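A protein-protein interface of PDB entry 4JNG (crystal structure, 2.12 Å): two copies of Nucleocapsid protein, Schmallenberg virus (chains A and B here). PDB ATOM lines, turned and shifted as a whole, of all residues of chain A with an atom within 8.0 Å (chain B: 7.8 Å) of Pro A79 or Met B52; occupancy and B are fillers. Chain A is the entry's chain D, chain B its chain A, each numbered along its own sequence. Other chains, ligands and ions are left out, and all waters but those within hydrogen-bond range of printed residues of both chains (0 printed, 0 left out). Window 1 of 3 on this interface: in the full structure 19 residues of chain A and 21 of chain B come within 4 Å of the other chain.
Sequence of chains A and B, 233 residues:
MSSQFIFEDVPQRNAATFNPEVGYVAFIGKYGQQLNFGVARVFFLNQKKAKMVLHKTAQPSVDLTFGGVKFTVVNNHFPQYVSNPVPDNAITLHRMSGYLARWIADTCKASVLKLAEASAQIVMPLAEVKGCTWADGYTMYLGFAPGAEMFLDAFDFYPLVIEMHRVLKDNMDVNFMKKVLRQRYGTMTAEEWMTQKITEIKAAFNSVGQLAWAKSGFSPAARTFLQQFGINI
Among the printed residues, merely in contact across the chains: Pro A79 with Met B52 (2.8 Å), Phe A7 with Asn B46 (3.7 Å), Phe A7 with Ala B50 (3.7 Å), Gln A4 with Val B53 (3.7 Å), Gln A80 with Met B52 (3.7 Å) and Gln A80 with Val B53 (3.7 Å).
Printed residues of chain B that touch a printed residue of chain A: Asn B46, Lys B49, Ala B50, Met B52, Val B53 and Lys B56. Hydrophobic or aromatic side chains of chain A within 4 Å of the printed part of chain B: Phe A7. Among the printed residues, 9 pairs touch across the chains.
OG1 of Thr B57 sits at hydrogen-bond distance from O of Val B53, at 2.7 Å.
NZ of Lys B56 is in hydrogen-bond range of OE1 of Gln A4 (2.8 Å). The side-chain amino group (NZ) of Lys B56 lies within hydrogen-bond range of the side-chain amide oxygen (OE1) of Gln A80. The side-chain amino group (NZ) of Lys B49 sits at hydrogen-bond distance from the backbone carbonyl oxygen (O) of Gln A80, at 2.9 Å.
Positions printed for both chains: 54, 55, 56, 57, 77 and 78. Of the 9 pairs that touch across the chains among the printed residues, none has its exchanged pair printed and touching as well.
Of the printed residues of chain B, Pro A79 touches Met B52. Of the printed residues of chain B, Gln A80 touches Lys B49, Met B52, Val B53 and Lys B56. Ser A83 touches none of the printed residues of chain B. Of the printed residues of chain A, Asn B46 touches Phe A7 (3.7 Å). Of the printed residues of chain A, Lys B49 touches Gln A80. Printed residues of chain A within 4 Å of Val B53: Gln A4 (3.7 Å) and Gln A80 (3.7 Å). His B55 touches none of the printed residues of chain A. Of the printed residues of chain A, Lys B56 touches Gln A4 and Gln A80.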
ATOM      1  N   GLN A   4      25.869  -8.941  18.583  1.00  0.00           N
ATOM      2  CA  GLN A   4      26.159  -8.716  17.165  1.00  0.00           C
ATOM      3  C   GLN A   4      26.871  -7.391  16.871  1.00  0.00           C
ATOM      4  O   GLN A   4      27.357  -7.188  15.760  1.00  0.00           O
ATOM      5  CB  GLN A   4      24.851  -8.757  16.364  1.00  0.00           C
ATOM      6  CG  GLN A   4      23.808  -7.746  16.836  1.00  0.00           C
ATOM      7  CD  GLN A   4      22.547  -7.743  15.996  1.00  0.00           C
ATOM      8  OE1 GLN A   4      22.520  -8.276  14.887  1.00  0.00           O
ATOM      9  NE2 GLN A   4      21.492  -7.136  16.524  1.00  0.00           N
ATOM     10  N   PHE A   7      32.773  -6.926  18.101  1.00  0.00           N
ATOM     11  CA  PHE A   7      33.657  -7.728  17.266  1.00  0.00           C
ATOM     12  C   PHE A   7      35.017  -7.913  17.951  1.00  0.00           C
ATOM     13  O   PHE A   7      35.611  -6.954  18.449  1.00  0.00           O
ATOM     14  CB  PHE A   7      33.839  -7.064  15.897  1.00  0.00           C
ATOM     15  CG  PHE A   7      32.542  -6.762  15.189  1.00  0.00           C
ATOM     16  CD1 PHE A   7      31.852  -5.584  15.441  1.00  0.00           C
ATOM     17  CD2 PHE A   7      32.011  -7.658  14.271  1.00  0.00           C
ATOM     18  CE1 PHE A   7      30.657  -5.306  14.795  1.00  0.00           C
ATOM     19  CE2 PHE A   7      30.816  -7.382  13.616  1.00  0.00           C
ATOM     20  CZ  PHE A   7      30.138  -6.207  13.880  1.00  0.00           C
ATOM     21  N   LEU A  54      17.865 -23.341   9.502  1.00  0.00           N
ATOM     22  CA  LEU A  54      19.038 -22.976  10.305  1.00  0.00           C
ATOM     23  C   LEU A  54      19.616 -21.622   9.891  1.00  0.00           C
ATOM     24  O   LEU A  54      20.188 -20.899  10.714  1.00  0.00           O
ATOM     25  CB  LEU A  54      20.131 -24.042  10.181  1.00  0.00           C
ATOM     26  CG  LEU A  54      20.040 -25.323  11.013  1.00  0.00           C
ATOM     27  CD1 LEU A  54      21.340 -26.106  10.895  1.00  0.00           C
ATOM     28  CD2 LEU A  54      19.758 -25.018  12.473  1.00  0.00           C
ATOM     29  N   HIS A  55      19.472 -21.302   8.607  1.00  0.00           N
ATOM     30  CA  HIS A  55      19.900 -20.026   8.043  1.00  0.00           C
ATOM     31  C   HIS A  55      19.316 -18.821   8.784  1.00  0.00           C
ATOM     32  O   HIS A  55      20.018 -17.834   8.993  1.00  0.00           O
ATOM     33  CB  HIS A  55      19.534 -19.989   6.550  1.00  0.00           C
ATOM     34  CG  HIS A  55      19.543 -18.622   5.939  1.00  0.00           C
ATOM     35  ND1 HIS A  55      20.547 -18.191   5.100  1.00  0.00           N
ATOM     36  CD2 HIS A  55      18.655 -17.602   6.016  1.00  0.00           C
ATOM     37  CE1 HIS A  55      20.283 -16.959   4.700  1.00  0.00           C
ATOM     38  NE2 HIS A  55      19.141 -16.580   5.243  1.00  0.00           N
ATOM     39  N   LYS A  56      18.047 -18.906   9.187  1.00  0.00           N
ATOM     40  CA  LYS A  56      17.341 -17.753   9.763  1.00  0.00           C
ATOM     41  C   LYS A  56      17.302 -17.705  11.291  1.00  0.00           C
ATOM     42  O   LYS A  56      16.891 -16.688  11.852  1.00  0.00           O
ATOM     43  CB  LYS A  56      15.888 -17.679   9.270  1.00  0.00           C
ATOM     44  CG  LYS A  56      15.648 -18.014   7.806  1.00  0.00           C
ATOM     45  CD  LYS A  56      15.014 -16.847   7.059  1.00  0.00           C
ATOM     46  CE  LYS A  56      14.163 -17.311   5.889  1.00  0.00           C
ATOM     47  NZ  LYS A  56      13.240 -16.236   5.429  1.00  0.00           N
ATOM     48  N   THR A  57      17.699 -18.783  11.965  1.00  0.00           N
ATOM     49  CA  THR A  57      17.542 -18.862  13.422  1.00  0.00           C
ATOM     50  C   THR A  57      18.841 -18.557  14.172  1.00  0.00           C
ATOM     51  O   THR A  57      19.927 -18.979  13.766  1.00  0.00           O
ATOM     52  CB  THR A  57      16.938 -20.215  13.864  1.00  0.00           C
ATOM     53  OG1 THR A  57      17.237 -21.224  12.894  1.00  0.00           O
ATOM     54  CG2 THR A  57      15.421 -20.098  13.993  1.00  0.00           C
ATOM     55  N   ASN A  75      25.563 -24.464  14.557  1.00  0.00           N
ATOM     56  CA  ASN A  75      25.061 -23.698  13.426  1.00  0.00           C
ATOM     57  C   ASN A  75      25.929 -22.503  13.053  1.00  0.00           C
ATOM     58  O   ASN A  75      25.985 -21.513  13.787  1.00  0.00           O
ATOM     59  CB  ASN A  75      23.634 -23.218  13.687  1.00  0.00           C
ATOM     60  CG  ASN A  75      23.030 -22.529  12.480  1.00  0.00           C
ATOM     61  OD1 ASN A  75      22.485 -21.436  12.581  1.00  0.00           O
ATOM     62  ND2 ASN A  75      23.134 -23.167  11.327  1.00  0.00           N
ATOM     63  N   ASN A  76      26.599 -22.605  11.906  1.00  0.00           N
ATOM     64  CA  ASN A  76      27.298 -21.475  11.297  1.00  0.00           C
ATOM     65  C   ASN A  76      26.556 -20.943  10.056  1.00  0.00           C
ATOM     66  O   ASN A  76      27.121 -20.174   9.283  1.00  0.00           O
ATOM     67  CB  ASN A  76      28.730 -21.875  10.908  1.00  0.00           C
ATOM     68  CG  ASN A  76      29.731 -21.731  12.048  1.00  0.00           C
ATOM     69  OD1 ASN A  76      30.883 -21.357  11.819  1.00  0.00           O
ATOM     70  ND2 ASN A  76      29.311 -22.038  13.272  1.00  0.00           N
ATOM     71  N   HIS A  77      25.303 -21.347   9.852  1.00  0.00           N
ATOM     72  CA  HIS A  77      24.537 -20.878   8.686  1.00  0.00           C
ATOM     73  C   HIS A  77      23.957 -19.485   8.880  1.00  0.00           C
ATOM     74  O   HIS A  77      23.836 -18.728   7.916  1.00  0.00           O
ATOM     75  CB  HIS A  77      23.395 -21.832   8.335  1.00  0.00           C
ATOM     76  CG  HIS A  77      23.847 -23.112   7.710  1.00  0.00           C
ATOM     77  ND1 HIS A  77      24.543 -24.081   8.400  1.00  0.00           N
ATOM     78  CD2 HIS A  77      23.698 -23.579   6.449  1.00  0.00           C
ATOM     79  CE1 HIS A  77      24.801 -25.092   7.589  1.00  0.00           C
ATOM     80  NE2 HIS A  77      24.299 -24.812   6.400  1.00  0.00           N
ATOM     81  N   PHE A  78      23.558 -19.166  10.111  1.00  0.00           N
ATOM     82  CA  PHE A  78      23.128 -17.813  10.459  1.00  0.00           C
ATOM     83  C   PHE A  78      24.242 -16.841  10.059  1.00  0.00           C
ATOM     84  O   PHE A  78      25.319 -16.877  10.660  1.00  0.00           O
ATOM     85  CB  PHE A  78      22.831 -17.718  11.958  1.00  0.00           C
ATOM     86  CG  PHE A  78      22.287 -16.384  12.393  1.00  0.00           C
ATOM     87  CD1 PHE A  78      21.077 -15.914  11.893  1.00  0.00           C
ATOM     88  CD2 PHE A  78      22.975 -15.607  13.317  1.00  0.00           C
ATOM     89  CE1 PHE A  78      20.572 -14.689  12.295  1.00  0.00           C
ATOM     90  CE2 PHE A  78      22.473 -14.382  13.724  1.00  0.00           C
ATOM     91  CZ  PHE A  78      21.271 -13.921  13.212  1.00  0.00           C
ATOM     92  N   PRO A  79      23.995 -15.976   9.045  1.00  0.00           N
ATOM     93  CA  PRO A  79      25.068 -15.220   8.376  1.00  0.00           C
ATOM     94  C   PRO A  79      25.774 -14.189   9.267  1.00  0.00           C
ATOM     95  O   PRO A  79      25.933 -13.036   8.885  1.00  0.00           O
ATOM     96  CB  PRO A  79      24.349 -14.536   7.194  1.00  0.00           C
ATOM     97  CG  PRO A  79      22.980 -15.126   7.143  1.00  0.00           C
ATOM     98  CD  PRO A  79      22.675 -15.568   8.537  1.00  0.00           C
ATOM     99  N   GLN A  80      26.207 -14.640  10.436  1.00  0.00           N
ATOM    100  CA  GLN A  80      26.912 -13.823  11.421  1.00  0.00           C
ATOM    101  C   GLN A  80      27.606 -14.744  12.441  1.00  0.00           C
ATOM    102  O   GLN A  80      28.587 -14.354  13.076  1.00  0.00           O
ATOM    103  CB  GLN A  80      25.957 -12.813  12.080  1.00  0.00           C
ATOM    104  CG  GLN A  80      26.027 -11.405  11.477  1.00  0.00           C
ATOM    105  CD  GLN A  80      24.662 -10.784  11.202  1.00  0.00           C
ATOM    106  OE1 GLN A  80      23.962 -10.361  12.122  1.00  0.00           O
ATOM    107  NE2 GLN A  80      24.289 -10.707   9.925  1.00  0.00           N
ATOM    108  N   TYR A  81      27.082 -15.963  12.586  1.00  0.00           N
ATOM    109  CA  TYR A  81      27.876 -17.102  13.035  1.00  0.00           C
ATOM    110  C   TYR A  81      28.693 -17.672  11.864  1.00  0.00           C
ATOM    111  O   TYR A  81      29.487 -18.591  12.060  1.00  0.00           O
ATOM    112  CB  TYR A  81      26.988 -18.220  13.597  1.00  0.00           C
ATOM    113  CG  TYR A  81      26.018 -17.814  14.689  1.00  0.00           C
ATOM    114  CD1 TYR A  81      26.322 -16.800  15.594  1.00  0.00           C
ATOM    115  CD2 TYR A  81      24.803 -18.479  14.837  1.00  0.00           C
ATOM    116  CE1 TYR A  81      25.432 -16.445  16.595  1.00  0.00           C
ATOM    117  CE2 TYR A  81      23.908 -18.133  15.834  1.00  0.00           C
ATOM    118  CZ  TYR A  81      24.226 -17.117  16.712  1.00  0.00           C
ATOM    119  OH  TYR A  81      23.337 -16.776  17.704  1.00  0.00           O
ATOM    120  N   VAL A  82      28.499 -17.125  10.659  1.00  0.00           N
ATOM    121  CA  VAL A  82      29.135 -17.620   9.425  1.00  0.00           C
ATOM    122  C   VAL A  82      30.655 -17.838   9.543  1.00  0.00           C
ATOM    123  O   VAL A  82      31.238 -18.559   8.735  1.00  0.00           O
ATOM    124  CB  VAL A  82      28.775 -16.719   8.209  1.00  0.00           C
ATOM    125  CG1 VAL A  82      29.437 -15.350   8.308  1.00  0.00           C
ATOM    126  CG2 VAL A  82      29.120 -17.398   6.892  1.00  0.00           C
ATOM    127  N   SER A  83      31.282 -17.206  10.538  1.00  0.00           N
ATOM    128  CA  SER A  83      32.579 -17.647  11.063  1.00  0.00           C
ATOM    129  C   SER A  83      32.441 -17.764  12.581  1.00  0.00           C
ATOM    130  O   SER A  83      31.767 -16.930  13.186  1.00  0.00           O
ATOM    131  CB  SER A  83      33.683 -16.651  10.714  1.00  0.00           C
ATOM    132  OG  SER A  83      33.781 -15.628  11.693  1.00  0.00           O
ATOM    133  N   ASN B  46      36.284  -7.754   9.926  1.00  0.00           N
ATOM    134  CA  ASN B  46      34.864  -7.808  10.274  1.00  0.00           C
ATOM    135  C   ASN B  46      34.036  -6.699   9.631  1.00  0.00           C
ATOM    136  O   ASN B  46      32.917  -6.416  10.062  1.00  0.00           O
ATOM    137  CB  ASN B  46      34.705  -7.767  11.789  1.00  0.00           C
ATOM    138  CG  ASN B  46      35.207  -9.027  12.451  1.00  0.00           C
ATOM    139  OD1 ASN B  46      36.375  -9.126  12.814  1.00  0.00           O
ATOM    140  ND2 ASN B  46      34.323 -10.000  12.615  1.00  0.00           N
ATOM    141  N   GLN B  47      34.581  -6.090   8.585  1.00  0.00           N
ATOM    142  CA  GLN B  47      33.990  -4.904   8.010  1.00  0.00           C
ATOM    143  C   GLN B  47      32.777  -5.262   7.148  1.00  0.00           C
ATOM    144  O   GLN B  47      31.769  -4.565   7.183  1.00  0.00           O
ATOM    145  CB  GLN B  47      35.017  -4.126   7.189  1.00  0.00           C
ATOM    146  CG  GLN B  47      34.425  -2.877   6.553  1.00  0.00           C
ATOM    147  CD  GLN B  47      35.406  -2.103   5.705  1.00  0.00           C
ATOM    148  OE1 GLN B  47      36.463  -2.604   5.335  1.00  0.00           O
ATOM    149  NE2 GLN B  47      35.041  -0.870   5.365  1.00  0.00           N
ATOM    150  N   LYS B  48      32.889  -6.338   6.376  1.00  0.00           N
ATOM    151  CA  LYS B  48      31.761  -6.874   5.625  1.00  0.00           C
ATOM    152  C   LYS B  48      30.641  -7.326   6.560  1.00  0.00           C
ATOM    153  O   LYS B  48      29.458  -7.067   6.298  1.00  0.00           O
ATOM    154  CB  LYS B  48      32.223  -8.028   4.732  1.00  0.00           C
ATOM    155  CG  LYS B  48      31.109  -8.769   4.002  1.00  0.00           C
ATOM    156  CD  LYS B  48      31.521  -9.143   2.585  1.00  0.00           C
ATOM    157  CE  LYS B  48      30.805 -10.391   2.094  1.00  0.00           C
ATOM    158  NZ  LYS B  48      31.105 -10.659   0.660  1.00  0.00           N
ATOM    159  N   LYS B  49      31.014  -7.996   7.646  1.00  0.00           N
ATOM    160  CA  LYS B  49      30.056  -8.464   8.642  1.00  0.00           C
ATOM    161  C   LYS B  49      29.310  -7.321   9.336  1.00  0.00           C
ATOM    162  O   LYS B  49      28.109  -7.416   9.584  1.00  0.00           O
ATOM    163  CB  LYS B  49      30.770  -9.322   9.697  1.00  0.00           C
ATOM    164  CG  LYS B  49      29.840  -9.996  10.689  1.00  0.00           C
ATOM    165  CD  LYS B  49      30.565 -11.052  11.499  1.00  0.00           C
ATOM    166  CE  LYS B  49      29.886 -11.283  12.840  1.00  0.00           C
ATOM    167  NZ  LYS B  49      30.577 -12.339  13.630  1.00  0.00           N
ATOM    168  N   ALA B  50      30.025  -6.250   9.672  1.00  0.00           N
ATOM    169  CA  ALA B  50      29.430  -5.119  10.386  1.00  0.00           C
ATOM    170  C   ALA B  50      28.420  -4.400   9.487  1.00  0.00           C
ATOM    171  O   ALA B  50      27.414  -3.862   9.942  1.00  0.00           O
ATOM    172  CB  ALA B  50      30.514  -4.156  10.835  1.00  0.00           C
ATOM    173  N   LYS B  51      28.728  -4.416   8.202  1.00  0.00           N
ATOM    174  CA  LYS B  51      27.934  -3.793   7.169  1.00  0.00           C
ATOM    175  C   LYS B  51      26.614  -4.557   6.994  1.00  0.00           C
ATOM    176  O   LYS B  51      25.556  -3.955   6.846  1.00  0.00           O
ATOM    177  CB  LYS B  51      28.794  -3.785   5.904  1.00  0.00           C
ATOM    178  CG  LYS B  51      28.132  -3.410   4.610  1.00  0.00           C
ATOM    179  CD  LYS B  51      29.113  -3.630   3.467  1.00  0.00           C
ATOM    180  CE  LYS B  51      29.890  -2.375   3.129  1.00  0.00           C
ATOM    181  NZ  LYS B  51      30.588  -2.578   1.831  1.00  0.00           N
ATOM    182  N   MET B  52      26.686  -5.884   7.053  1.00  0.00           N
ATOM    183  CA  MET B  52      25.494  -6.736   7.049  1.00  0.00           C
ATOM    184  C   MET B  52      24.643  -6.506   8.288  1.00  0.00           C
ATOM    185  O   MET B  52      23.414  -6.463   8.205  1.00  0.00           O
ATOM    186  CB  MET B  52      25.895  -8.204   7.015  1.00  0.00           C
ATOM    187  CG  MET B  52      26.568  -8.647   5.730  1.00  0.00           C
ATOM    188  SD  MET B  52      27.746  -9.982   6.019  1.00  0.00           S
ATOM    189  CE  MET B  52      26.924 -10.946   7.285  1.00  0.00           C
ATOM    190  N   VAL B  53      25.296  -6.381   9.438  1.00  0.00           N
ATOM    191  CA  VAL B  53      24.602  -6.048  10.674  1.00  0.00           C
ATOM    192  C   VAL B  53      23.831  -4.746  10.439  1.00  0.00           C
ATOM    193  O   VAL B  53      22.591  -4.728  10.488  1.00  0.00           O
ATOM    194  CB  VAL B  53      25.583  -5.937  11.866  1.00  0.00           C
ATOM    195  CG1 VAL B  53      24.921  -5.305  13.082  1.00  0.00           C
ATOM    196  CG2 VAL B  53      26.121  -7.310  12.239  1.00  0.00           C
ATOM    197  N   LEU B  54      24.562  -3.681  10.117  1.00  0.00           N
ATOM    198  CA  LEU B  54      23.968  -2.353   9.876  1.00  0.00           C
ATOM    199  C   LEU B  54      22.860  -2.356   8.809  1.00  0.00           C
ATOM    200  O   LEU B  54      21.870  -1.636   8.935  1.00  0.00           O
ATOM    201  CB  LEU B  54      25.065  -1.337   9.499  1.00  0.00           C
ATOM    202  CG  LEU B  54      25.577  -0.398  10.605  1.00  0.00           C
ATOM    203  CD1 LEU B  54      25.699  -1.078  11.958  1.00  0.00           C
ATOM    204  CD2 LEU B  54      26.901   0.228  10.203  1.00  0.00           C
ATOM    205  N   HIS B  55      23.035  -3.169   7.772  1.00  0.00           N
ATOM    206  CA  HIS B  55      22.054  -3.288   6.701  1.00  0.00           C
ATOM    207  C   HIS B  55      20.705  -3.822   7.192  1.00  0.00           C
ATOM    208  O   HIS B  55      19.663  -3.494   6.618  1.00  0.00           O
ATOM    209  CB  HIS B  55      22.595  -4.181   5.581  1.00  0.00           C
ATOM    210  CG  HIS B  55      21.604  -4.439   4.496  1.00  0.00           C
ATOM    211  ND1 HIS B  55      21.540  -3.679   3.348  1.00  0.00           N
ATOM    212  CD2 HIS B  55      20.606  -5.348   4.402  1.00  0.00           C
ATOM    213  CE1 HIS B  55      20.556  -4.118   2.588  1.00  0.00           C
ATOM    214  NE2 HIS B  55      19.970  -5.128   3.205  1.00  0.00           N
ATOM    215  N   LYS B  56      20.730  -4.636   8.246  1.00  0.00           N
ATOM    216  CA  LYS B  56      19.517  -5.203   8.828  1.00  0.00           C
ATOM    217  C   LYS B  56      19.111  -4.544  10.157  1.00  0.00           C
ATOM    218  O   LYS B  56      18.134  -4.965  10.791  1.00  0.00           O
ATOM    219  CB  LYS B  56      19.669  -6.728   8.983  1.00  0.00           C
ATOM    220  CG  LYS B  56      20.239  -7.224  10.310  1.00  0.00           C
ATOM    221  CD  LYS B  56      20.628  -8.699  10.226  1.00  0.00           C
ATOM    222  CE  LYS B  56      20.265  -9.461  11.493  1.00  0.00           C
ATOM    223  NZ  LYS B  56      20.933  -8.902  12.698  1.00  0.00           N
ATOM    224  N   THR B  57      19.829  -3.497  10.563  1.00  0.00           N
ATOM    225  CA  THR B  57      19.588  -2.869  11.860  1.00  0.00           C
ATOM    226  C   THR B  57      18.898  -1.520  11.709  1.00  0.00           C
ATOM    227  O   THR B  57      19.372  -0.650  10.981  1.00  0.00           O
ATOM    228  CB  THR B  57      20.900  -2.706  12.648  1.00  0.00           C
ATOM    229  OG1 THR B  57      21.506  -3.989  12.807  1.00  0.00           O
ATOM    230  CG2 THR B  57      20.639  -2.102  14.008  1.00  0.00           C
ATOM    231  N   HIS B  77      23.131   2.257   5.935  1.00  0.00           N
ATOM    232  CA  HIS B  77      23.059   1.003   5.187  1.00  0.00           C
ATOM    233  C   HIS B  77      21.647   0.423   5.143  1.00  0.00           C
ATOM    234  O   HIS B  77      21.227  -0.120   4.120  1.00  0.00           O
ATOM    235  CB  HIS B  77      23.999  -0.023   5.794  1.00  0.00           C
ATOM    236  CG  HIS B  77      25.440   0.275   5.553  1.00  0.00           C
ATOM    237  ND1 HIS B  77      26.063  -0.005   4.359  1.00  0.00           N
ATOM    238  CD2 HIS B  77      26.383   0.825   6.353  1.00  0.00           C
ATOM    239  CE1 HIS B  77      27.332   0.359   4.432  1.00  0.00           C
ATOM    240  NE2 HIS B  77      27.550   0.866   5.632  1.00  0.00           N
ATOM    241  N   PHE B  78      20.945   0.500   6.272  1.00  0.00           N
ATOM    242  CA  PHE B  78      19.548   0.096   6.337  1.00  0.00           C
ATOM    243  C   PHE B  78      18.792   0.895   5.261  1.00  0.00           C
ATOM    244  O   PHE B  78      18.880   2.126   5.234  1.00  0.00           O
ATOM    245  CB  PHE B  78      18.987   0.351   7.742  1.00  0.00           C
ATOM    246  CG  PHE B  78      17.566  -0.115   7.933  1.00  0.00           C
ATOM    247  CD1 PHE B  78      17.285  -1.458   8.130  1.00  0.00           C
ATOM    248  CD2 PHE B  78      16.510   0.796   7.931  1.00  0.00           C
ATOM    249  CE1 PHE B  78      15.976  -1.888   8.307  1.00  0.00           C
ATOM    250  CE2 PHE B  78      15.200   0.372   8.109  1.00  0.00           C
ATOM    251  CZ  PHE B  78      14.933  -0.972   8.295  1.00  0.00           C
ATOM    252  N   LEU B  93      30.665   3.500   8.367  1.00  0.00           N
ATOM    253  CA  LEU B  93      31.557   2.375   8.204  1.00  0.00           C
ATOM    254  C   LEU B  93      32.595   2.668   7.132  1.00  0.00           C
ATOM    255  O   LEU B  93      33.795   2.363   7.296  1.00  0.00           O
ATOM    256  CB  LEU B  93      30.755   1.124   7.849  1.00  0.00           C
ATOM    257  CG  LEU B  93      31.179  -0.212   8.465  1.00  0.00           C
ATOM    258  CD1 LEU B  93      31.680  -0.064   9.894  1.00  0.00           C
ATOM    259  CD2 LEU B  93      29.998  -1.170   8.418  1.00  0.00           C
